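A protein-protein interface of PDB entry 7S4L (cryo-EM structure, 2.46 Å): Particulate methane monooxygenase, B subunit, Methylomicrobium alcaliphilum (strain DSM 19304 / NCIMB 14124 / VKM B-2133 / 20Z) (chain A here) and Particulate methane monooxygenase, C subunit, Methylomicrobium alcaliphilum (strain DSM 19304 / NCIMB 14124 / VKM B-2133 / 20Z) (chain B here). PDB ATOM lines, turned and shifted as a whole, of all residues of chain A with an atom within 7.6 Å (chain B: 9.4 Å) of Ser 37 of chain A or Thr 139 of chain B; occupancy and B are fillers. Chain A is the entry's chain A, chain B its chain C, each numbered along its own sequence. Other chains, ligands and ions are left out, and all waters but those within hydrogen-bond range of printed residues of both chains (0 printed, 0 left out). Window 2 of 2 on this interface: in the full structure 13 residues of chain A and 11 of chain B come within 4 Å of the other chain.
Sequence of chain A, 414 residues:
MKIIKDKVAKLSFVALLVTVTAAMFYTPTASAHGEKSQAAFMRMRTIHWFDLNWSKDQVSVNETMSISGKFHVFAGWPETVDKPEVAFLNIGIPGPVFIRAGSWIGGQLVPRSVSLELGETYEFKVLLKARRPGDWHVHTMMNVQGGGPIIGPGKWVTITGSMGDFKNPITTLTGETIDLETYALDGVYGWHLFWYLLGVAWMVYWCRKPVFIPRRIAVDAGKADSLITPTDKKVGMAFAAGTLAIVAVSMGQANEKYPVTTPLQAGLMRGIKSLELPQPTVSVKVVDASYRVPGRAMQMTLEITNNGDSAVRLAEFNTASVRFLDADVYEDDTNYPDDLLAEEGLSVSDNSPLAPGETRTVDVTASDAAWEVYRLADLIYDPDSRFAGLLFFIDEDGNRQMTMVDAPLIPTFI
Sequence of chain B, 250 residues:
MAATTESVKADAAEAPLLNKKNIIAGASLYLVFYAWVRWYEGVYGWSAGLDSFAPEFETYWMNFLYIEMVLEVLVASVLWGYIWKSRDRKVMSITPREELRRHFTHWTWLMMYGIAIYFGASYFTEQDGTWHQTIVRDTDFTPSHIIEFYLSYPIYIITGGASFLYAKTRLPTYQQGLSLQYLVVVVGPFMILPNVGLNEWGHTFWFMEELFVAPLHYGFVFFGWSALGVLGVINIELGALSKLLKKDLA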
ATOM      1  N   HIS A  33     -10.710  26.571  28.928  1.00  0.00           N
ATOM      2  CA  HIS A  33     -10.443  25.803  27.685  1.00  0.00           C
ATOM      3  C   HIS A  33      -9.483  24.662  28.029  1.00  0.00           C
ATOM      4  O   HIS A  33      -9.643  23.564  27.458  1.00  0.00           O
ATOM      5  CB  HIS A  33      -9.829  26.738  26.640  1.00  0.00           C
ATOM      6  CG  HIS A  33     -10.628  26.960  25.398  1.00  0.00           C
ATOM      7  ND1 HIS A  33     -11.990  27.250  25.388  1.00  0.00           N
ATOM      8  CD2 HIS A  33     -10.237  26.967  24.109  1.00  0.00           C
ATOM      9  CE1 HIS A  33     -12.366  27.467  24.142  1.00  0.00           C
ATOM     10  NE2 HIS A  33     -11.333  27.246  23.350  1.00  0.00           N
ATOM     11  N   GLY A  34      -8.539  24.913  28.941  1.00  0.00           N
ATOM     12  CA  GLY A  34      -7.541  23.892  29.313  1.00  0.00           C
ATOM     13  C   GLY A  34      -7.986  23.053  30.499  1.00  0.00           C
ATOM     14  O   GLY A  34      -7.156  22.274  31.004  1.00  0.00           O
ATOM     15  N   GLU A  35      -9.240  23.206  30.937  1.00  0.00           N
ATOM     16  CA  GLU A  35      -9.763  22.350  32.035  1.00  0.00           C
ATOM     17  C   GLU A  35      -9.711  20.881  31.601  1.00  0.00           C
ATOM     18  O   GLU A  35      -9.519  20.026  32.482  1.00  0.00           O
ATOM     19  CB  GLU A  35     -11.165  22.794  32.468  1.00  0.00           C
ATOM     20  CG  GLU A  35     -12.272  22.446  31.489  1.00  0.00           C
ATOM     21  CD  GLU A  35     -12.381  23.388  30.304  1.00  0.00           C
ATOM     22  OE1 GLU A  35     -12.037  24.573  30.468  1.00  0.00           O
ATOM     23  OE2 GLU A  35     -12.792  22.932  29.220  1.00  0.00           O
ATOM     24  N   LYS A  36      -9.845  20.602  30.300  1.00  0.00           N
ATOM     25  CA  LYS A  36      -9.881  19.214  29.859  1.00  0.00           C
ATOM     26  C   LYS A  36      -8.584  18.477  30.148  1.00  0.00           C
ATOM     27  O   LYS A  36      -8.572  17.244  30.132  1.00  0.00           O
ATOM     28  CB  LYS A  36     -10.187  19.142  28.367  1.00  0.00           C
ATOM     29  CG  LYS A  36     -11.556  19.654  27.992  1.00  0.00           C
ATOM     30  CD  LYS A  36     -11.798  19.508  26.506  1.00  0.00           C
ATOM     31  CE  LYS A  36     -13.062  20.219  26.082  1.00  0.00           C
ATOM     32  NZ  LYS A  36     -13.239  20.197  24.608  1.00  0.00           N
ATOM     33  N   SER A  37      -7.497  19.193  30.413  1.00  0.00           N
ATOM     34  CA  SER A  37      -6.215  18.554  30.654  1.00  0.00           C
ATOM     35  C   SER A  37      -5.887  18.399  32.130  1.00  0.00           C
ATOM     36  O   SER A  37      -4.854  17.811  32.457  1.00  0.00           O
ATOM     37  CB  SER A  37      -5.098  19.342  29.973  1.00  0.00           C
ATOM     38  OG  SER A  37      -4.843  20.547  30.668  1.00  0.00           O
ATOM     39  N   GLN A  38      -6.723  18.911  33.023  1.00  0.00           N
ATOM     40  CA  GLN A  38      -6.466  18.786  34.447  1.00  0.00           C
ATOM     41  C   GLN A  38      -6.933  17.435  34.964  1.00  0.00           C
ATOM     42  O   GLN A  38      -7.860  16.826  34.426  1.00  0.00           O
ATOM     43  CB  GLN A  38      -7.164  19.900  35.219  1.00  0.00           C
ATOM     44  CG  GLN A  38      -6.478  21.233  35.119  1.00  0.00           C
ATOM     45  CD  GLN A  38      -7.203  22.306  35.886  1.00  0.00           C
ATOM     46  OE1 GLN A  38      -8.428  22.376  35.866  1.00  0.00           O
ATOM     47  NE2 GLN A  38      -6.451  23.150  36.571  1.00  0.00           N
ATOM     48  N   ALA A  39      -6.278  16.989  36.038  1.00  0.00           N
ATOM     49  CA  ALA A  39      -6.620  15.695  36.666  1.00  0.00           C
ATOM     50  C   ALA A  39      -8.130  15.602  36.901  1.00  0.00           C
ATOM     51  O   ALA A  39      -8.697  16.545  37.483  1.00  0.00           O
ATOM     52  CB  ALA A  39      -5.844  15.605  37.952  1.00  0.00           C
ATOM     53  N   ALA A  40      -8.753  14.500  36.474  1.00  0.00           N
ATOM     54  CA  ALA A  40     -10.221  14.346  36.608  1.00  0.00           C
ATOM     55  C   ALA A  40     -10.645  14.452  38.079  1.00  0.00           C
ATOM     56  O   ALA A  40     -11.614  15.177  38.350  1.00  0.00           O
ATOM     57  CB  ALA A  40     -10.661  13.044  35.990  1.00  0.00           C
ATOM     58  N   ARG A  43     -10.587  18.067  39.339  1.00  0.00           N
ATOM     59  CA  ARG A  43     -11.748  18.840  38.830  1.00  0.00           C
ATOM     60  C   ARG A  43     -12.996  18.472  39.636  1.00  0.00           C
ATOM     61  O   ARG A  43     -13.936  19.287  39.659  1.00  0.00           O
ATOM     62  CB  ARG A  43     -11.967  18.543  37.347  1.00  0.00           C
ATOM     63  CG  ARG A  43     -10.876  19.096  36.445  1.00  0.00           C
ATOM     64  CD  ARG A  43     -11.275  18.901  35.000  1.00  0.00           C
ATOM     65  NE  ARG A  43     -10.725  17.679  34.440  1.00  0.00           N
ATOM     66  CZ  ARG A  43     -11.038  17.210  33.242  1.00  0.00           C
ATOM     67  NH1 ARG A  43     -10.491  16.092  32.800  1.00  0.00           N
ATOM     68  NH2 ARG A  43     -11.895  17.872  32.486  1.00  0.00           N
ATOM     69  N   PRO A 149      -5.014  26.959  38.908  1.00  0.00           N
ATOM     70  CA  PRO A 149      -6.280  27.477  38.391  1.00  0.00           C
ATOM     71  C   PRO A 149      -7.397  26.471  38.565  1.00  0.00           C
ATOM     72  O   PRO A 149      -7.235  25.294  38.236  1.00  0.00           O
ATOM     73  CB  PRO A 149      -5.970  27.728  36.917  1.00  0.00           C
ATOM     74  CG  PRO A 149      -4.952  26.710  36.597  1.00  0.00           C
ATOM     75  CD  PRO A 149      -4.125  26.504  37.832  1.00  0.00           C
ATOM     76  N   ILE A 151     -10.967  26.050  37.196  1.00  0.00           N
ATOM     77  CA  ILE A 151     -11.753  26.632  36.118  1.00  0.00           C
ATOM     78  C   ILE A 151     -13.186  26.141  36.214  1.00  0.00           C
ATOM     79  O   ILE A 151     -13.433  24.937  36.327  1.00  0.00           O
ATOM     80  CB  ILE A 151     -11.146  26.280  34.753  1.00  0.00           C
ATOM     81  CG1 ILE A 151      -9.645  26.538  34.785  1.00  0.00           C
ATOM     82  CG2 ILE A 151     -11.798  27.089  33.667  1.00  0.00           C
ATOM     83  CD1 ILE A 151      -8.906  25.907  33.654  1.00  0.00           C
ATOM     84  N   TYR A 374     -15.071  15.537  27.929  1.00  0.00           N
ATOM     85  CA  TYR A 374     -14.324  16.366  28.911  1.00  0.00           C
ATOM     86  C   TYR A 374     -13.296  15.510  29.655  1.00  0.00           C
ATOM     87  O   TYR A 374     -12.945  15.885  30.786  1.00  0.00           O
ATOM     88  CB  TYR A 374     -15.283  17.157  29.803  1.00  0.00           C
ATOM     89  CG  TYR A 374     -15.637  18.507  29.234  1.00  0.00           C
ATOM     90  CD1 TYR A 374     -16.499  18.624  28.156  1.00  0.00           C
ATOM     91  CD2 TYR A 374     -15.084  19.666  29.750  1.00  0.00           C
ATOM     92  CE1 TYR A 374     -16.816  19.857  27.614  1.00  0.00           C
ATOM     93  CE2 TYR A 374     -15.394  20.909  29.222  1.00  0.00           C
ATOM     94  CZ  TYR A 374     -16.261  21.006  28.149  1.00  0.00           C
ATOM     95  OH  TYR A 374     -16.570  22.227  27.626  1.00  0.00           O
ATOM     96  N   ARG A 375     -12.846  14.407  29.049  1.00  0.00           N
ATOM     97  CA  ARG A 375     -11.768  13.557  29.627  1.00  0.00           C
ATOM     98  C   ARG A 375     -12.028  13.180  31.089  1.00  0.00           C
ATOM     99  O   ARG A 375     -11.039  12.973  31.811  1.00  0.00           O
ATOM    100  CB  ARG A 375     -10.398  14.208  29.410  1.00  0.00           C
ATOM    101  CG  ARG A 375     -10.116  14.569  27.958  1.00  0.00           C
ATOM    102  CD  ARG A 375      -8.656  14.871  27.684  1.00  0.00           C
ATOM    103  NE  ARG A 375      -8.489  16.149  27.008  1.00  0.00           N
ATOM    104  CZ  ARG A 375      -7.354  16.839  26.965  1.00  0.00           C
ATOM    105  NH1 ARG A 375      -6.275  16.374  27.569  1.00  0.00           N
ATOM    106  NH2 ARG A 375      -7.304  17.993  26.324  1.00  0.00           N
ATOM    107  N   LEU B  50      -6.512  27.219  20.024  1.00  0.00           N
ATOM    108  CA  LEU B  50      -6.712  27.444  21.450  1.00  0.00           C
ATOM    109  C   LEU B  50      -6.984  26.148  22.197  1.00  0.00           C
ATOM    110  O   LEU B  50      -6.633  26.030  23.376  1.00  0.00           O
ATOM    111  CB  LEU B  50      -7.866  28.417  21.669  1.00  0.00           C
ATOM    112  CG  LEU B  50      -7.533  29.896  21.538  1.00  0.00           C
ATOM    113  CD1 LEU B  50      -8.797  30.724  21.446  1.00  0.00           C
ATOM    114  CD2 LEU B  50      -6.691  30.339  22.713  1.00  0.00           C
ATOM    115  N   ASP B  51      -7.637  25.191  21.533  1.00  0.00           N
ATOM    116  CA  ASP B  51      -8.014  23.935  22.231  1.00  0.00           C
ATOM    117  C   ASP B  51      -7.256  22.756  21.623  1.00  0.00           C
ATOM    118  O   ASP B  51      -7.263  22.637  20.385  1.00  0.00           O
ATOM    119  CB  ASP B  51      -9.526  23.698  22.188  1.00  0.00           C
ATOM    120  CG  ASP B  51     -10.028  22.835  23.333  1.00  0.00           C
ATOM    121  OD1 ASP B  51     -11.148  22.302  23.219  1.00  0.00           O
ATOM    122  OD2 ASP B  51      -9.294  22.704  24.332  1.00  0.00           O
ATOM    123  N   SER B  52      -6.641  21.917  22.463  1.00  0.00           N
ATOM    124  CA  SER B  52      -5.979  20.689  21.948  1.00  0.00           C
ATOM    125  C   SER B  52      -7.043  19.846  21.246  1.00  0.00           C
ATOM    126  O   SER B  52      -6.697  19.238  20.218  1.00  0.00           O
ATOM    127  CB  SER B  52      -5.304  19.927  23.054  1.00  0.00           C
ATOM    128  OG  SER B  52      -3.906  20.182  23.058  1.00  0.00           O
ATOM    129  N   PHE B  53      -8.264  19.794  21.795  1.00  0.00           N
ATOM    130  CA  PHE B  53      -9.405  19.101  21.138  1.00  0.00           C
ATOM    131  C   PHE B  53      -8.952  17.853  20.381  1.00  0.00           C
ATOM    132  O   PHE B  53      -8.447  16.912  21.031  1.00  0.00           O
ATOM    133  CB  PHE B  53     -10.064  20.047  20.132  1.00  0.00           C
ATOM    134  CG  PHE B  53     -11.528  20.310  20.367  1.00  0.00           C
ATOM    135  CD1 PHE B  53     -12.098  21.516  19.993  1.00  0.00           C
ATOM    136  CD2 PHE B  53     -12.336  19.352  20.956  1.00  0.00           C
ATOM    137  CE1 PHE B  53     -13.446  21.760  20.208  1.00  0.00           C
ATOM    138  CE2 PHE B  53     -13.684  19.596  21.168  1.00  0.00           C
ATOM    139  CZ  PHE B  53     -14.235  20.800  20.794  1.00  0.00           C
ATOM    140  N   PHE B  57      -6.900  21.224  15.751  1.00  0.00           N
ATOM    141  CA  PHE B  57      -5.550  21.352  16.353  1.00  0.00           C
ATOM    142  C   PHE B  57      -4.585  20.398  15.641  1.00  0.00           C
ATOM    143  O   PHE B  57      -3.555  20.877  15.148  1.00  0.00           O
ATOM    144  CB  PHE B  57      -5.577  21.090  17.857  1.00  0.00           C
ATOM    145  CG  PHE B  57      -4.348  21.570  18.583  1.00  0.00           C
ATOM    146  CD1 PHE B  57      -4.162  22.917  18.842  1.00  0.00           C
ATOM    147  CD2 PHE B  57      -3.369  20.680  18.995  1.00  0.00           C
ATOM    148  CE1 PHE B  57      -3.031  23.364  19.506  1.00  0.00           C
ATOM    149  CE2 PHE B  57      -2.238  21.128  19.657  1.00  0.00           C
ATOM    150  CZ  PHE B  57      -2.071  22.469  19.911  1.00  0.00           C
ATOM    151  N   HIS B 132       1.354  32.716  27.934  1.00  0.00           N
ATOM    152  CA  HIS B 132       0.851  32.105  29.202  1.00  0.00           C
ATOM    153  C   HIS B 132       0.067  33.155  29.948  1.00  0.00           C
ATOM    154  O   HIS B 132      -1.051  32.856  30.424  1.00  0.00           O
ATOM    155  CB  HIS B 132       2.012  31.798  30.153  1.00  0.00           C
ATOM    156  CG  HIS B 132       2.971  30.932  29.444  1.00  0.00           C
ATOM    157  ND1 HIS B 132       2.498  30.186  28.429  1.00  0.00           N
ATOM    158  CD2 HIS B 132       4.305  30.716  29.523  1.00  0.00           C
ATOM    159  CE1 HIS B 132       3.485  29.563  27.898  1.00  0.00           C
ATOM    160  NE2 HIS B 132       4.612  29.809  28.536  1.00  0.00           N
ATOM    161  N   ILE B 135      -3.914  33.286  28.418  1.00  0.00           N
ATOM    162  CA  ILE B 135      -4.851  32.216  28.720  1.00  0.00           C
ATOM    163  C   ILE B 135      -4.104  30.924  28.989  1.00  0.00           C
ATOM    164  O   ILE B 135      -4.264  30.294  30.039  1.00  0.00           O
ATOM    165  CB  ILE B 135      -5.854  32.023  27.572  1.00  0.00           C
ATOM    166  CG1 ILE B 135      -6.632  30.716  27.751  1.00  0.00           C
ATOM    167  CG2 ILE B 135      -5.128  32.029  26.237  1.00  0.00           C
ATOM    168  CD1 ILE B 135      -7.663  30.751  28.857  1.00  0.00           C
ATOM    169  N   VAL B 136      -3.275  30.527  28.034  1.00  0.00           N
ATOM    170  CA  VAL B 136      -2.903  29.125  27.902  1.00  0.00           C
ATOM    171  C   VAL B 136      -2.051  28.714  29.097  1.00  0.00           C
ATOM    172  O   VAL B 136      -0.873  29.066  29.188  1.00  0.00           O
ATOM    173  CB  VAL B 136      -2.175  28.869  26.585  1.00  0.00           C
ATOM    174  CG1 VAL B 136      -1.787  27.404  26.478  1.00  0.00           C
ATOM    175  CG2 VAL B 136      -3.072  29.273  25.442  1.00  0.00           C
ATOM    176  N   ARG B 137      -2.650  27.956  30.011  1.00  0.00           N
ATOM    177  CA  ARG B 137      -1.881  27.234  31.009  1.00  0.00           C
ATOM    178  C   ARG B 137      -1.138  26.093  30.331  1.00  0.00           C
ATOM    179  O   ARG B 137      -1.706  25.348  29.530  1.00  0.00           O
ATOM    180  CB  ARG B 137      -2.789  26.692  32.107  1.00  0.00           C
ATOM    181  CG  ARG B 137      -2.793  27.514  33.379  1.00  0.00           C
ATOM    182  CD  ARG B 137      -3.760  28.677  33.292  1.00  0.00           C
ATOM    183  NE  ARG B 137      -4.347  28.815  31.967  1.00  0.00           N
ATOM    184  CZ  ARG B 137      -5.546  28.357  31.641  1.00  0.00           C
ATOM    185  NH1 ARG B 137      -6.277  27.725  32.543  1.00  0.00           N
ATOM    186  NH2 ARG B 137      -6.011  28.522  30.414  1.00  0.00           N
ATOM    187  N   ASP B 138       0.141  25.948  30.674  1.00  0.00           N
ATOM    188  CA  ASP B 138       0.992  25.009  29.957  1.00  0.00           C
ATOM    189  C   ASP B 138       0.491  23.575  30.031  1.00  0.00           C
ATOM    190  O   ASP B 138       1.099  22.704  29.402  1.00  0.00           O
ATOM    191  CB  ASP B 138       2.420  25.082  30.495  1.00  0.00           C
ATOM    192  CG  ASP B 138       3.003  26.463  30.377  1.00  0.00           C
ATOM    193  OD1 ASP B 138       2.709  27.135  29.370  1.00  0.00           O
ATOM    194  OD2 ASP B 138       3.760  26.874  31.278  1.00  0.00           O
ATOM    195  N   THR B 139      -0.609  23.314  30.745  1.00  0.00           N
ATOM    196  CA  THR B 139      -0.994  21.947  31.071  1.00  0.00           C
ATOM    197  C   THR B 139      -1.065  21.097  29.808  1.00  0.00           C
ATOM    198  O   THR B 139      -1.961  21.257  28.973  1.00  0.00           O
ATOM    199  CB  THR B 139      -2.342  21.921  31.805  1.00  0.00           C
ATOM    200  OG1 THR B 139      -2.447  23.065  32.662  1.00  0.00           O
ATOM    201  CG2 THR B 139      -2.466  20.665  32.646  1.00  0.00           C
ATOM    202  N   ASP B 140      -0.089  20.202  29.671  1.00  0.00           N
ATOM    203  CA  ASP B 140       0.009  19.222  28.600  1.00  0.00           C
ATOM    204  C   ASP B 140       0.396  19.816  27.249  1.00  0.00           C
ATOM    205  O   ASP B 140       0.829  19.071  26.364  1.00  0.00           O
ATOM    206  CB  ASP B 140      -1.322  18.465  28.467  1.00  0.00           C
ATOM    207  CG  ASP B 140      -1.518  17.851  27.088  1.00  0.00           C
ATOM    208  OD1 ASP B 140      -1.083  16.701  26.875  1.00  0.00           O
ATOM    209  OD2 ASP B 140      -2.115  18.517  26.218  1.00  0.00           O
ATOM    210  N   PHE B 141       0.316  21.136  27.079  1.00  0.00           N
ATOM    211  CA  PHE B 141       0.798  21.684  25.815  1.00  0.00           C
ATOM    212  C   PHE B 141       0.605  23.182  25.628  1.00  0.00           C
ATOM    213  O   PHE B 141       0.025  23.866  26.476  1.00  0.00           O
ATOM    214  CB  PHE B 141       0.149  20.981  24.627  1.00  0.00           C
ATOM    215  CG  PHE B 141       1.018  20.967  23.413  1.00  0.00           C
ATOM    216  CD1 PHE B 141       0.560  21.449  22.206  1.00  0.00           C
ATOM    217  CD2 PHE B 141       2.309  20.488  23.494  1.00  0.00           C
ATOM    218  CE1 PHE B 141       1.372  21.436  21.105  1.00  0.00           C
ATOM    219  CE2 PHE B 141       3.121  20.470  22.396  1.00  0.00           C
ATOM    220  CZ  PHE B 141       2.656  20.943  21.199  1.00  0.00           C
ATOM    221  N   THR B 142       1.107  23.679  24.498  1.00  0.00           N
ATOM    222  CA  THR B 142       0.851  24.998  23.948  1.00  0.00           C
ATOM    223  C   THR B 142       1.178  24.972  22.465  1.00  0.00           C
ATOM    224  O   THR B 142       2.002  24.160  22.027  1.00  0.00           O
ATOM    225  CB  THR B 142       1.688  26.075  24.648  1.00  0.00           C
ATOM    226  OG1 THR B 142       1.278  26.179  26.016  1.00  0.00           O
ATOM    227  CG2 THR B 142       1.509  27.411  23.973  1.00  0.00           C
ATOM    228  N   PRO B 143       0.422  25.680  21.563  1.00  0.00           N
ATOM    229  CA  PRO B 143       0.820  25.804  20.149  1.00  0.00           C
ATOM    230  C   PRO B 143       1.872  26.900  19.913  1.00  0.00           C
ATOM    231  O   PRO B 143       2.479  26.903  18.861  1.00  0.00           O
ATOM    232  CB  PRO B 143      -0.455  26.234  19.414  1.00  0.00           C
ATOM    233  CG  PRO B 143      -1.197  27.040  20.434  1.00  0.00           C
ATOM    234  CD  PRO B 143      -0.954  26.260  21.705  1.00  0.00           C
ATOM    235  N   HIS B 145       4.401  26.587  21.323  1.00  0.00           N
ATOM    236  CA  HIS B 145       5.534  25.717  21.735  1.00  0.00           C
ATOM    237  C   HIS B 145       6.101  24.979  20.533  1.00  0.00           C
ATOM    238  O   HIS B 145       7.327  24.781  20.478  1.00  0.00           O
ATOM    239  CB  HIS B 145       5.022  24.639  22.666  1.00  0.00           C
ATOM    240  CG  HIS B 145       5.272  25.035  24.062  1.00  0.00           C
ATOM    241  ND1 HIS B 145       5.742  24.137  24.986  1.00  0.00           N
ATOM    242  CD2 HIS B 145       5.180  26.251  24.641  1.00  0.00           C
ATOM    243  CE1 HIS B 145       5.928  24.757  26.117  1.00  0.00           C
ATOM    244  NE2 HIS B 145       5.557  26.121  25.935  1.00  0.00           N
ATOM    245  N   GLU B 200       8.035  22.041  32.028  1.00  0.00           N
ATOM    246  CA  GLU B 200       7.040  21.009  31.787  1.00  0.00           C
ATOM    247  C   GLU B 200       7.191  19.881  32.796  1.00  0.00           C
ATOM    248  O   GLU B 200       6.326  19.010  32.863  1.00  0.00           O
ATOM    249  CB  GLU B 200       7.095  20.425  30.363  1.00  0.00           C
ATOM    250  N   HIS B 203       6.993  22.789  35.640  1.00  0.00           N
ATOM    251  CA  HIS B 203       5.632  23.278  35.475  1.00  0.00           C
ATOM    252  C   HIS B 203       4.595  22.244  35.877  1.00  0.00           C
ATOM    253  O   HIS B 203       3.395  22.506  35.746  1.00  0.00           O
ATOM    254  CB  HIS B 203       5.386  23.691  34.022  1.00  0.00           C
ATOM    255  CG  HIS B 203       5.972  25.018  33.660  1.00  0.00           C
ATOM    256  ND1 HIS B 203       6.727  25.211  32.524  1.00  0.00           N
ATOM    257  CD2 HIS B 203       5.914  26.219  34.282  1.00  0.00           C
ATOM    258  CE1 HIS B 203       7.108  26.475  32.461  1.00  0.00           C
ATOM    259  NE2 HIS B 203       6.628  27.107  33.516  1.00  0.00           N
ATOM    260  N   THR B 204       5.032  21.081  36.351  1.00  0.00           N
ATOM    261  CA  THR B 204       4.144  19.964  36.649  1.00  0.00           C
ATOM    262  C   THR B 204       4.721  19.194  37.825  1.00  0.00           C
ATOM    263  O   THR B 204       5.765  18.552  37.694  1.00  0.00           O
ATOM    264  CB  THR B 204       3.996  19.054  35.427  1.00  0.00           C
ATOM    265  OG1 THR B 204       3.410  19.793  34.349  1.00  0.00           O
ATOM    266  CG2 THR B 204       3.136  17.856  35.750  1.00  0.00           C
ATOM    267  N   PHE B 205       4.035  19.238  38.963  1.00  0.00           N
ATOM    268  CA  PHE B 205       4.470  18.698  40.243  1.00  0.00           C
ATOM    269  C   PHE B 205       5.473  19.633  40.922  1.00  0.00           C
ATOM    270  O   PHE B 205       5.755  19.455  42.108  1.00  0.00           O
ATOM    271  CB  PHE B 205       5.085  17.288  40.112  1.00  0.00           C
ATOM    272  CG  PHE B 205       6.060  16.932  41.196  1.00  0.00           C
ATOM    273  CD1 PHE B 205       5.623  16.370  42.380  1.00  0.00           C
ATOM    274  CD2 PHE B 205       7.416  17.156  41.028  1.00  0.00           C
ATOM    275  CE1 PHE B 205       6.515  16.043  43.376  1.00  0.00           C
ATOM    276  CE2 PHE B 205       8.310  16.833  42.021  1.00  0.00           C
ATOM    277  CZ  PHE B 205       7.861  16.276  43.197  1.00  0.00           C
ATOM    278  N   PHE B 207       5.243  23.235  39.834  1.00  0.00           N
ATOM    279  CA  PHE B 207       4.908  24.353  38.967  1.00  0.00           C
ATOM    280  C   PHE B 207       5.102  25.692  39.663  1.00  0.00           C
ATOM    281  O   PHE B 207       5.184  25.784  40.890  1.00  0.00           O
ATOM    282  CB  PHE B 207       3.465  24.226  38.489  1.00  0.00           C
ATOM    283  CG  PHE B 207       2.488  23.995  39.599  1.00  0.00           C
ATOM    284  CD1 PHE B 207       2.143  22.710  39.977  1.00  0.00           C
ATOM    285  CD2 PHE B 207       1.929  25.062  40.274  1.00  0.00           C
ATOM    286  CE1 PHE B 207       1.252  22.495  41.001  1.00  0.00           C
ATOM    287  CE2 PHE B 207       1.040  24.852  41.300  1.00  0.00           C
ATOM    288  CZ  PHE B 207       0.703  23.565  41.665  1.00  0.00           C
ATOM    289  N   GLU B 209       3.630  29.651  38.216  1.00  0.00           N
ATOM    290  CA  GLU B 209       3.032  30.312  37.063  1.00  0.00           C
ATOM    291  C   GLU B 209       3.718  31.638  36.764  1.00  0.00           C
ATOM    292  O   GLU B 209       3.062  32.680  36.648  1.00  0.00           O
ATOM    293  CB  GLU B 209       1.536  30.525  37.290  1.00  0.00           C
ATOM    294  CG  GLU B 209       0.721  29.238  37.398  1.00  0.00           C
ATOM    295  CD  GLU B 209       1.067  28.404  38.616  1.00  0.00           C
ATOM    296  OE1 GLU B 209       0.809  27.183  38.598  1.00  0.00           O
ATOM    297  OE2 GLU B 209       1.611  28.969  39.588  1.00  0.00           O
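NZ of Lys 36 of chain A lies within salt-bridge range of OD1 of Asp 51 of chain B, at 3.3 Å. The backbone carbonyl oxygen of Thr 139 of chain B sits close to the side-chain hydroxyl of Ser 37 of chain A (3.4 Å). The backbone carbonyl oxygen (O) of His 33 of chain A lies close to the side-chain carboxylate (OD2) of Asp 51 of chain B, at 3.3 Å.
Leu 50 of chain B touches His 33 of chain A. Lys 36 of chain A touches Phe 53 of chain B. CG of Arg 137 of chain B touches CG of Pro 149 of chain A (3.96 Å). Arg 137 of chain B touches Ile 151 of chain A.
Of the 22 printed residues of chain B, 5 touch a printed residue of chain A. Printed residues of chain B that touch a printed residue of chain A: Leu 50, Asp 51, Phe 53, Arg 137 and Thr 139. Hydrophobic or aromatic side chains of chain B within 4 Å of the printed part of chain A: Leu 50 and Phe 53. Along chain B the printed residues that touch a printed residue of chain A span positions 50 to 139. Of the 13 printed residues of chain A, 5 touch a printed residue of chain B.
Of the printed residues of chain B, Ser 37 of chain A touches Thr 139. Of chain A, only Ser 37 (3.1 Å) comes within 4 Å of Thr 139 of chain B. Printed residues of chain A within 4 Å of Leu 50 of chain B: His 33. Of the printed residues of chain B, Pro 149 of chain A touches Arg 137 (3.96 Å). Of the printed residues of chain A, Asp 51 of chain B touches His 33 and Lys 36. The nearest printed residue of chain B that does not touch Pro 149 of chain A is Glu 209 of chain B (5.0 Å).
The backbone NH of His 33 of chain A is in hydrogen-bond range of the side-chain carboxylate of Glu 35 of chain A, at 2.9 Å. The backbone carbonyl oxygen of Gly 34 of chain A is in hydrogen-bond range of the side-chain hydroxyl of Ser 37 of chain A. The backbone carbonyl oxygen (O) of Lys 36 of chain A sits at hydrogen-bond distance from the guanidinium group (NH1) of Arg 43 of chain A. The guanidinium group of Arg 375 of chain A lies within hydrogen-bond range of the backbone carbonyl oxygen of Lys 36 of chain A (3.3 Å). The side-chain amide nitrogen of Gln 38 of chain A lies within hydrogen-bond range of the backbone carbonyl oxygen of Pro 149 of chain A (2.8 Å). O of Ile 135 of chain B sits at hydrogen-bond distance from NE of Arg 137 of chain B (2.4 Å).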
